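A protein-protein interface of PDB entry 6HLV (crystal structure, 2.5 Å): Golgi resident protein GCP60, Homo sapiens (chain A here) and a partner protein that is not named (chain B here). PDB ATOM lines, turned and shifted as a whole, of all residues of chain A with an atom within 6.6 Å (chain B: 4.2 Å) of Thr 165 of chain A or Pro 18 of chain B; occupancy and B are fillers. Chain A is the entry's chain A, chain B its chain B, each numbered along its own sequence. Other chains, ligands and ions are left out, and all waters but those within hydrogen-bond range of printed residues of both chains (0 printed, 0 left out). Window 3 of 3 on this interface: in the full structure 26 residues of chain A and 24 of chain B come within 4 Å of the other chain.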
ATOM      1  N   HIS A  48     -15.800   9.341 -35.614  1.00  0.00           N
ATOM      2  CA  HIS A  48     -15.996   8.690 -34.326  1.00  0.00           C
ATOM      3  C   HIS A  48     -16.185   9.748 -33.239  1.00  0.00           C
ATOM      4  O   HIS A  48     -16.078  10.945 -33.504  1.00  0.00           O
ATOM      5  CB  HIS A  48     -14.809   7.776 -34.006  1.00  0.00           C
ATOM      6  CG  HIS A  48     -15.076   6.804 -32.897  1.00  0.00           C
ATOM      7  ND1 HIS A  48     -16.280   6.156 -32.752  1.00  0.00           N
ATOM      8  CD2 HIS A  48     -14.291   6.384 -31.876  1.00  0.00           C
ATOM      9  CE1 HIS A  48     -16.228   5.370 -31.687  1.00  0.00           C
ATOM     10  NE2 HIS A  48     -15.034   5.491 -31.142  1.00  0.00           N
ATOM     11  N   GLU A  49     -16.460   9.301 -32.016  1.00  0.00           N
ATOM     12  CA  GLU A  49     -16.774  10.202 -30.914  1.00  0.00           C
ATOM     13  C   GLU A  49     -15.532  10.841 -30.298  1.00  0.00           C
ATOM     14  O   GLU A  49     -14.431  10.292 -30.369  1.00  0.00           O
ATOM     15  CB  GLU A  49     -17.558   9.451 -29.835  1.00  0.00           C
ATOM     16  CG  GLU A  49     -18.966   9.046 -30.260  1.00  0.00           C
ATOM     17  CD  GLU A  49     -19.073   7.584 -30.667  1.00  0.00           C
ATOM     18  OE1 GLU A  49     -18.601   6.711 -29.907  1.00  0.00           O
ATOM     19  OE2 GLU A  49     -19.636   7.306 -31.747  1.00  0.00           O
ATOM     20  N   GLY A  51     -12.772  12.138 -27.624  1.00  0.00           N
ATOM     21  CA  GLY A  51     -12.097  11.513 -26.503  1.00  0.00           C
ATOM     22  C   GLY A  51     -11.502  10.165 -26.855  1.00  0.00           C
ATOM     23  O   GLY A  51     -10.606   9.679 -26.167  1.00  0.00           O
ATOM     24  N   SER A  52     -11.992   9.562 -27.933  1.00  0.00           N
ATOM     25  CA  SER A  52     -11.473   8.279 -28.377  1.00  0.00           C
ATOM     26  C   SER A  52     -10.085   8.481 -28.959  1.00  0.00           C
ATOM     27  O   SER A  52      -9.582   9.602 -29.006  1.00  0.00           O
ATOM     28  CB  SER A  52     -12.394   7.642 -29.416  1.00  0.00           C
ATOM     29  OG  SER A  52     -13.692   7.433 -28.890  1.00  0.00           O
ATOM     30  N   TYR A  53      -9.472   7.390 -29.401  1.00  0.00           N
ATOM     31  CA  TYR A  53      -8.155   7.444 -30.015  1.00  0.00           C
ATOM     32  C   TYR A  53      -8.175   6.748 -31.363  1.00  0.00           C
ATOM     33  O   TYR A  53      -8.815   5.713 -31.519  1.00  0.00           O
ATOM     34  CB  TYR A  53      -7.108   6.793 -29.111  1.00  0.00           C
ATOM     35  CG  TYR A  53      -6.566   7.702 -28.035  1.00  0.00           C
ATOM     36  CD1 TYR A  53      -7.377   8.155 -27.006  1.00  0.00           C
ATOM     37  CD2 TYR A  53      -5.235   8.099 -28.042  1.00  0.00           C
ATOM     38  CE1 TYR A  53      -6.881   8.985 -26.017  1.00  0.00           C
ATOM     39  CE2 TYR A  53      -4.730   8.928 -27.059  1.00  0.00           C
ATOM     40  CZ  TYR A  53      -5.557   9.367 -26.048  1.00  0.00           C
ATOM     41  OH  TYR A  53      -5.060  10.193 -25.067  1.00  0.00           O
ATOM     42  N   LEU A  54      -7.489   7.336 -32.335  1.00  0.00           N
ATOM     43  CA  LEU A  54      -7.228   6.663 -33.598  1.00  0.00           C
ATOM     44  C   LEU A  54      -5.834   6.072 -33.541  1.00  0.00           C
ATOM     45  O   LEU A  54      -4.900   6.731 -33.093  1.00  0.00           O
ATOM     46  CB  LEU A  54      -7.344   7.622 -34.783  1.00  0.00           C
ATOM     47  CG  LEU A  54      -7.083   6.978 -36.150  1.00  0.00           C
ATOM     48  CD1 LEU A  54      -8.274   6.141 -36.583  1.00  0.00           C
ATOM     49  CD2 LEU A  54      -6.750   8.019 -37.203  1.00  0.00           C
ATOM     50  N   PHE A  55      -5.706   4.825 -33.980  1.00  0.00           N
ATOM     51  CA  PHE A  55      -4.405   4.189 -34.129  1.00  0.00           C
ATOM     52  C   PHE A  55      -4.190   3.874 -35.595  1.00  0.00           C
ATOM     53  O   PHE A  55      -5.104   3.413 -36.272  1.00  0.00           O
ATOM     54  CB  PHE A  55      -4.312   2.917 -33.287  1.00  0.00           C
ATOM     55  CG  PHE A  55      -4.421   3.161 -31.813  1.00  0.00           C
ATOM     56  CD1 PHE A  55      -5.645   3.093 -31.178  1.00  0.00           C
ATOM     57  CD2 PHE A  55      -3.298   3.465 -31.064  1.00  0.00           C
ATOM     58  CE1 PHE A  55      -5.750   3.319 -29.823  1.00  0.00           C
ATOM     59  CE2 PHE A  55      -3.396   3.694 -29.709  1.00  0.00           C
ATOM     60  CZ  PHE A  55      -4.624   3.621 -29.087  1.00  0.00           C
ATOM     61  N   TYR A 136      -9.144  11.921 -30.332  1.00  0.00           N
ATOM     62  CA  TYR A 136     -10.176  12.637 -31.073  1.00  0.00           C
ATOM     63  C   TYR A 136     -10.473  13.994 -30.437  1.00  0.00           C
ATOM     64  O   TYR A 136     -10.933  14.053 -29.297  1.00  0.00           O
ATOM     65  CB  TYR A 136     -11.458  11.805 -31.141  1.00  0.00           C
ATOM     66  CG  TYR A 136     -11.459  10.764 -32.237  1.00  0.00           C
ATOM     67  CD1 TYR A 136     -10.796   9.555 -32.076  1.00  0.00           C
ATOM     68  CD2 TYR A 136     -12.128  10.989 -33.430  1.00  0.00           C
ATOM     69  CE1 TYR A 136     -10.797   8.602 -33.076  1.00  0.00           C
ATOM     70  CE2 TYR A 136     -12.134  10.043 -34.437  1.00  0.00           C
ATOM     71  CZ  TYR A 136     -11.467   8.851 -34.254  1.00  0.00           C
ATOM     72  OH  TYR A 136     -11.474   7.907 -35.256  1.00  0.00           O
ATOM     73  N   TYR A 163      -7.099   1.239 -36.222  1.00  0.00           N
ATOM     74  CA  TYR A 163      -8.055   0.931 -35.163  1.00  0.00           C
ATOM     75  C   TYR A 163      -8.579   2.213 -34.531  1.00  0.00           C
ATOM     76  O   TYR A 163      -7.993   3.280 -34.710  1.00  0.00           O
ATOM     77  CB  TYR A 163      -7.427   0.092 -34.048  1.00  0.00           C
ATOM     78  CG  TYR A 163      -6.817  -1.230 -34.436  1.00  0.00           C
ATOM     79  CD1 TYR A 163      -7.548  -2.406 -34.342  1.00  0.00           C
ATOM     80  CD2 TYR A 163      -5.495  -1.312 -34.842  1.00  0.00           C
ATOM     81  CE1 TYR A 163      -6.987  -3.622 -34.670  1.00  0.00           C
ATOM     82  CE2 TYR A 163      -4.924  -2.523 -35.169  1.00  0.00           C
ATOM     83  CZ  TYR A 163      -5.675  -3.675 -35.080  1.00  0.00           C
ATOM     84  OH  TYR A 163      -5.107  -4.883 -35.407  1.00  0.00           O
ATOM     85  N   TYR A 164      -9.675   2.110 -33.785  1.00  0.00           N
ATOM     86  CA  TYR A 164     -10.002   3.137 -32.801  1.00  0.00           C
ATOM     87  C   TYR A 164     -10.466   2.483 -31.507  1.00  0.00           C
ATOM     88  O   TYR A 164     -10.807   1.303 -31.487  1.00  0.00           O
ATOM     89  CB  TYR A 164     -11.062   4.125 -33.325  1.00  0.00           C
ATOM     90  CG  TYR A 164     -12.468   3.584 -33.553  1.00  0.00           C
ATOM     91  CD1 TYR A 164     -13.201   2.997 -32.525  1.00  0.00           C
ATOM     92  CD2 TYR A 164     -13.082   3.717 -34.789  1.00  0.00           C
ATOM     93  CE1 TYR A 164     -14.479   2.523 -32.736  1.00  0.00           C
ATOM     94  CE2 TYR A 164     -14.365   3.248 -35.007  1.00  0.00           C
ATOM     95  CZ  TYR A 164     -15.058   2.654 -33.977  1.00  0.00           C
ATOM     96  OH  TYR A 164     -16.335   2.186 -34.186  1.00  0.00           O
ATOM     97  N   THR A 165     -10.481   3.264 -30.431  1.00  0.00           N
ATOM     98  CA  THR A 165     -10.998   2.801 -29.150  1.00  0.00           C
ATOM     99  C   THR A 165     -12.495   3.055 -29.058  1.00  0.00           C
ATOM    100  O   THR A 165     -12.979   4.100 -29.491  1.00  0.00           O
ATOM    101  CB  THR A 165     -10.310   3.505 -27.972  1.00  0.00           C
ATOM    102  OG1 THR A 165     -10.640   4.898 -27.992  1.00  0.00           O
ATOM    103  CG2 THR A 165      -8.808   3.341 -28.050  1.00  0.00           C
ATOM    104  N   ARG A 166     -13.228   2.099 -28.497  1.00  0.00           N
ATOM    105  CA  ARG A 166     -14.652   2.284 -28.252  1.00  0.00           C
ATOM    106  C   ARG A 166     -14.871   3.313 -27.150  1.00  0.00           C
ATOM    107  O   ARG A 166     -14.553   3.063 -25.988  1.00  0.00           O
ATOM    108  CB  ARG A 166     -15.318   0.962 -27.869  1.00  0.00           C
ATOM    109  CG  ARG A 166     -15.789   0.130 -29.049  1.00  0.00           C
ATOM    110  CD  ARG A 166     -16.846  -0.875 -28.616  1.00  0.00           C
ATOM    111  NE  ARG A 166     -17.400  -1.624 -29.742  1.00  0.00           N
ATOM    112  CZ  ARG A 166     -16.921  -2.781 -30.191  1.00  0.00           C
ATOM    113  NH1 ARG A 166     -15.862  -3.344 -29.619  1.00  0.00           N
ATOM    114  NH2 ARG A 166     -17.501  -3.380 -31.223  1.00  0.00           N
ATOM    115  N   PRO B  16     -11.904   0.609 -19.114  1.00  0.00           N
ATOM    116  CA  PRO B  16     -10.531   0.741 -19.613  1.00  0.00           C
ATOM    117  C   PRO B  16     -10.316   2.080 -20.322  1.00  0.00           C
ATOM    118  O   PRO B  16     -10.741   2.234 -21.467  1.00  0.00           O
ATOM    119  CB  PRO B  16     -10.390  -0.438 -20.587  1.00  0.00           C
ATOM    120  CG  PRO B  16     -11.456  -1.399 -20.187  1.00  0.00           C
ATOM    121  CD  PRO B  16     -12.586  -0.569 -19.674  1.00  0.00           C
ATOM    122  N   PRO B  17      -9.681   3.047 -19.641  1.00  0.00           N
ATOM    123  CA  PRO B  17      -9.467   4.364 -20.250  1.00  0.00           C
ATOM    124  C   PRO B  17      -8.696   4.277 -21.566  1.00  0.00           C
ATOM    125  O   PRO B  17      -7.722   3.528 -21.638  1.00  0.00           O
ATOM    126  CB  PRO B  17      -8.654   5.115 -19.190  1.00  0.00           C
ATOM    127  CG  PRO B  17      -8.982   4.439 -17.911  1.00  0.00           C
ATOM    128  CD  PRO B  17      -9.179   2.996 -18.256  1.00  0.00           C
ATOM    129  N   PRO B  18      -9.130   5.019 -22.599  1.00  0.00           N
ATOM    130  CA  PRO B  18      -8.386   5.000 -23.863  1.00  0.00           C
ATOM    131  C   PRO B  18      -6.953   5.493 -23.698  1.00  0.00           C
ATOM    132  O   PRO B  18      -6.053   5.025 -24.396  1.00  0.00           O
ATOM    133  CB  PRO B  18      -9.190   5.946 -24.757  1.00  0.00           C
ATOM    134  CG  PRO B  18     -10.558   5.939 -24.185  1.00  0.00           C
ATOM    135  CD  PRO B  18     -10.369   5.808 -22.708  1.00  0.00           C
ATOM    136  N   GLU B  19      -6.753   6.429 -22.776  1.00  0.00           N
ATOM    137  CA  GLU B  19      -5.429   6.972 -22.509  1.00  0.00           C
ATOM    138  C   GLU B  19      -4.479   5.872 -22.051  1.00  0.00           C
ATOM    139  O   GLU B  19      -3.282   5.913 -22.331  1.00  0.00           O
ATOM    140  CB  GLU B  19      -5.508   8.075 -21.452  1.00  0.00           C
ATOM    141  CG  GLU B  19      -6.541   9.149 -21.753  1.00  0.00           C
ATOM    142  N   CYS B  20      -5.024   4.884 -21.348  1.00  0.00           N
ATOM    143  CA  CYS B  20      -4.228   3.779 -20.829  1.00  0.00           C
ATOM    144  C   CYS B  20      -3.924   2.753 -21.917  1.00  0.00           C
ATOM    145  O   CYS B  20      -2.825   2.200 -21.963  1.00  0.00           O
ATOM    146  CB  CYS B  20      -4.948   3.116 -19.655  1.00  0.00           C
ATOM    147  SG  CYS B  20      -5.142   4.207 -18.222  1.00  0.00           S
ATOM    148  N   ILE B  21      -4.898   2.497 -22.785  1.00  0.00           N
ATOM    149  CA  ILE B  21      -4.671   1.662 -23.959  1.00  0.00           C
ATOM    150  C   ILE B  21      -3.554   2.266 -24.799  1.00  0.00           C
ATOM    151  O   ILE B  21      -2.658   1.564 -25.268  1.00  0.00           O
ATOM    152  CB  ILE B  21      -5.935   1.529 -24.833  1.00  0.00           C
ATOM    153  CG1 ILE B  21      -7.037   0.766 -24.090  1.00  0.00           C
ATOM    154  CG2 ILE B  21      -5.603   0.838 -26.151  1.00  0.00           C
ATOM    155  CD1 ILE B  21      -6.724  -0.700 -23.835  1.00  0.00           C
ATOM    156  N   ASN B  22      -3.624   3.580 -24.980  1.00  0.00           N
ATOM    157  CA  ASN B  22      -2.646   4.299 -25.780  1.00  0.00           C
ATOM    158  C   ASN B  22      -1.244   4.159 -25.208  1.00  0.00           C
ATOM    159  O   ASN B  22      -0.305   3.818 -25.927  1.00  0.00           O
ATOM    160  CB  ASN B  22      -3.030   5.776 -25.875  1.00  0.00           C
ATOM    161  CG  ASN B  22      -2.087   6.567 -26.752  1.00  0.00           C
ATOM    162  OD1 ASN B  22      -2.047   6.376 -27.966  1.00  0.00           O
ATOM    163  ND2 ASN B  22      -1.328   7.468 -26.144  1.00  0.00           N
ATOM    164  N   TRP B  42     -11.972  -3.529 -26.694  1.00  0.00           N
ATOM    165  CA  TRP B  42     -11.442  -2.207 -26.386  1.00  0.00           C
ATOM    166  C   TRP B  42     -11.112  -1.429 -27.656  1.00  0.00           C
ATOM    167  O   TRP B  42     -11.375  -0.230 -27.735  1.00  0.00           O
ATOM    168  CB  TRP B  42     -10.207  -2.331 -25.497  1.00  0.00           C
ATOM    169  CG  TRP B  42     -10.493  -3.031 -24.207  1.00  0.00           C
ATOM    170  CD1 TRP B  42     -11.712  -3.184 -23.611  1.00  0.00           C
ATOM    171  CD2 TRP B  42      -9.546  -3.687 -23.358  1.00  0.00           C
ATOM    172  NE1 TRP B  42     -11.582  -3.892 -22.442  1.00  0.00           N
ATOM    173  CE2 TRP B  42     -10.261  -4.212 -22.261  1.00  0.00           C
ATOM    174  CE3 TRP B  42      -8.163  -3.881 -23.414  1.00  0.00           C
ATOM    175  CZ2 TRP B  42      -9.642  -4.915 -21.233  1.00  0.00           C
ATOM    176  CZ3 TRP B  42      -7.550  -4.579 -22.392  1.00  0.00           C
ATOM    177  CH2 TRP B  42      -8.288  -5.088 -21.316  1.00  0.00           C
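N of Arg 166 of chain A sits at hydrogen-bond distance from O of Trp 42 of chain B (3.1 Å).
The backbone carbonyl oxygen (O) of Thr 165 of chain A is in hydrogen-bond range of a ring nitrogen (NE2) of His 48 of chain A (3.0 Å).
The side-chain hydroxyl (OG) of Ser 52 of chain A lies within hydrogen-bond range of the backbone carbonyl oxygen (O) of Thr 165 of chain A, 3.5 Å away.
N of Phe 55 of chain A is in hydrogen-bond range of O of Tyr 163 of chain A (2.9 Å).
The backbone NH (N) of Tyr 53 of chain A is in hydrogen-bond range of the side-chain hydroxyl (OG1) of Thr 165 of chain A (3.1 Å).
CD1 of Tyr 53 of chain A touches CB of Pro 18 of chain B (3.6 Å).
Glu 19 of chain B touches Tyr 53 of chain A.
Tyr 53 of chain A touches Asn 22 of chain B (CE2 to CG, 3.6 Å).
Asn 22 of chain B touches Phe 55 of chain A.
Pro 18 of chain B touches Thr 165 of chain A.
Thr 165 of chain A touches Trp 42 of chain B (CA to O, 3.4 Å).
Printed residues of chain B within 4 Å of Tyr 53 of chain A: Pro 18 (3.6 Å), Glu 19 (3.8 Å) and Asn 22 (3.6 Å).
Thr 165 of chain A touches two residues of chain B.
Of the printed residues of chain A, Pro 18 of chain B touches Tyr 53 and Thr 165.
Printed residues of chain A within 4 Å of Trp 42 of chain B: Thr 165 and Arg 166.
The nearest printed residue of chain B that does not touch Thr 165 of chain A is Ile 21 of chain B (4.5 Å).
Printed residues of chain B that touch a printed residue of chain A: Pro 18, Glu 19, Asn 22 and Trp 42.
Hydrophobic or aromatic side chains of chain B that line the printed part of chain A: Pro 18.
Hydrophobic or aromatic side chains of chain A that line the printed part of chain B: Tyr 53 and Phe 55.
Among the printed residues, 7 pairs touch across the chains.
Among the printed residues, no Asp or Glu carboxylate lies within 4 Å of a Lys or Arg side-chain nitrogen of the other chain.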
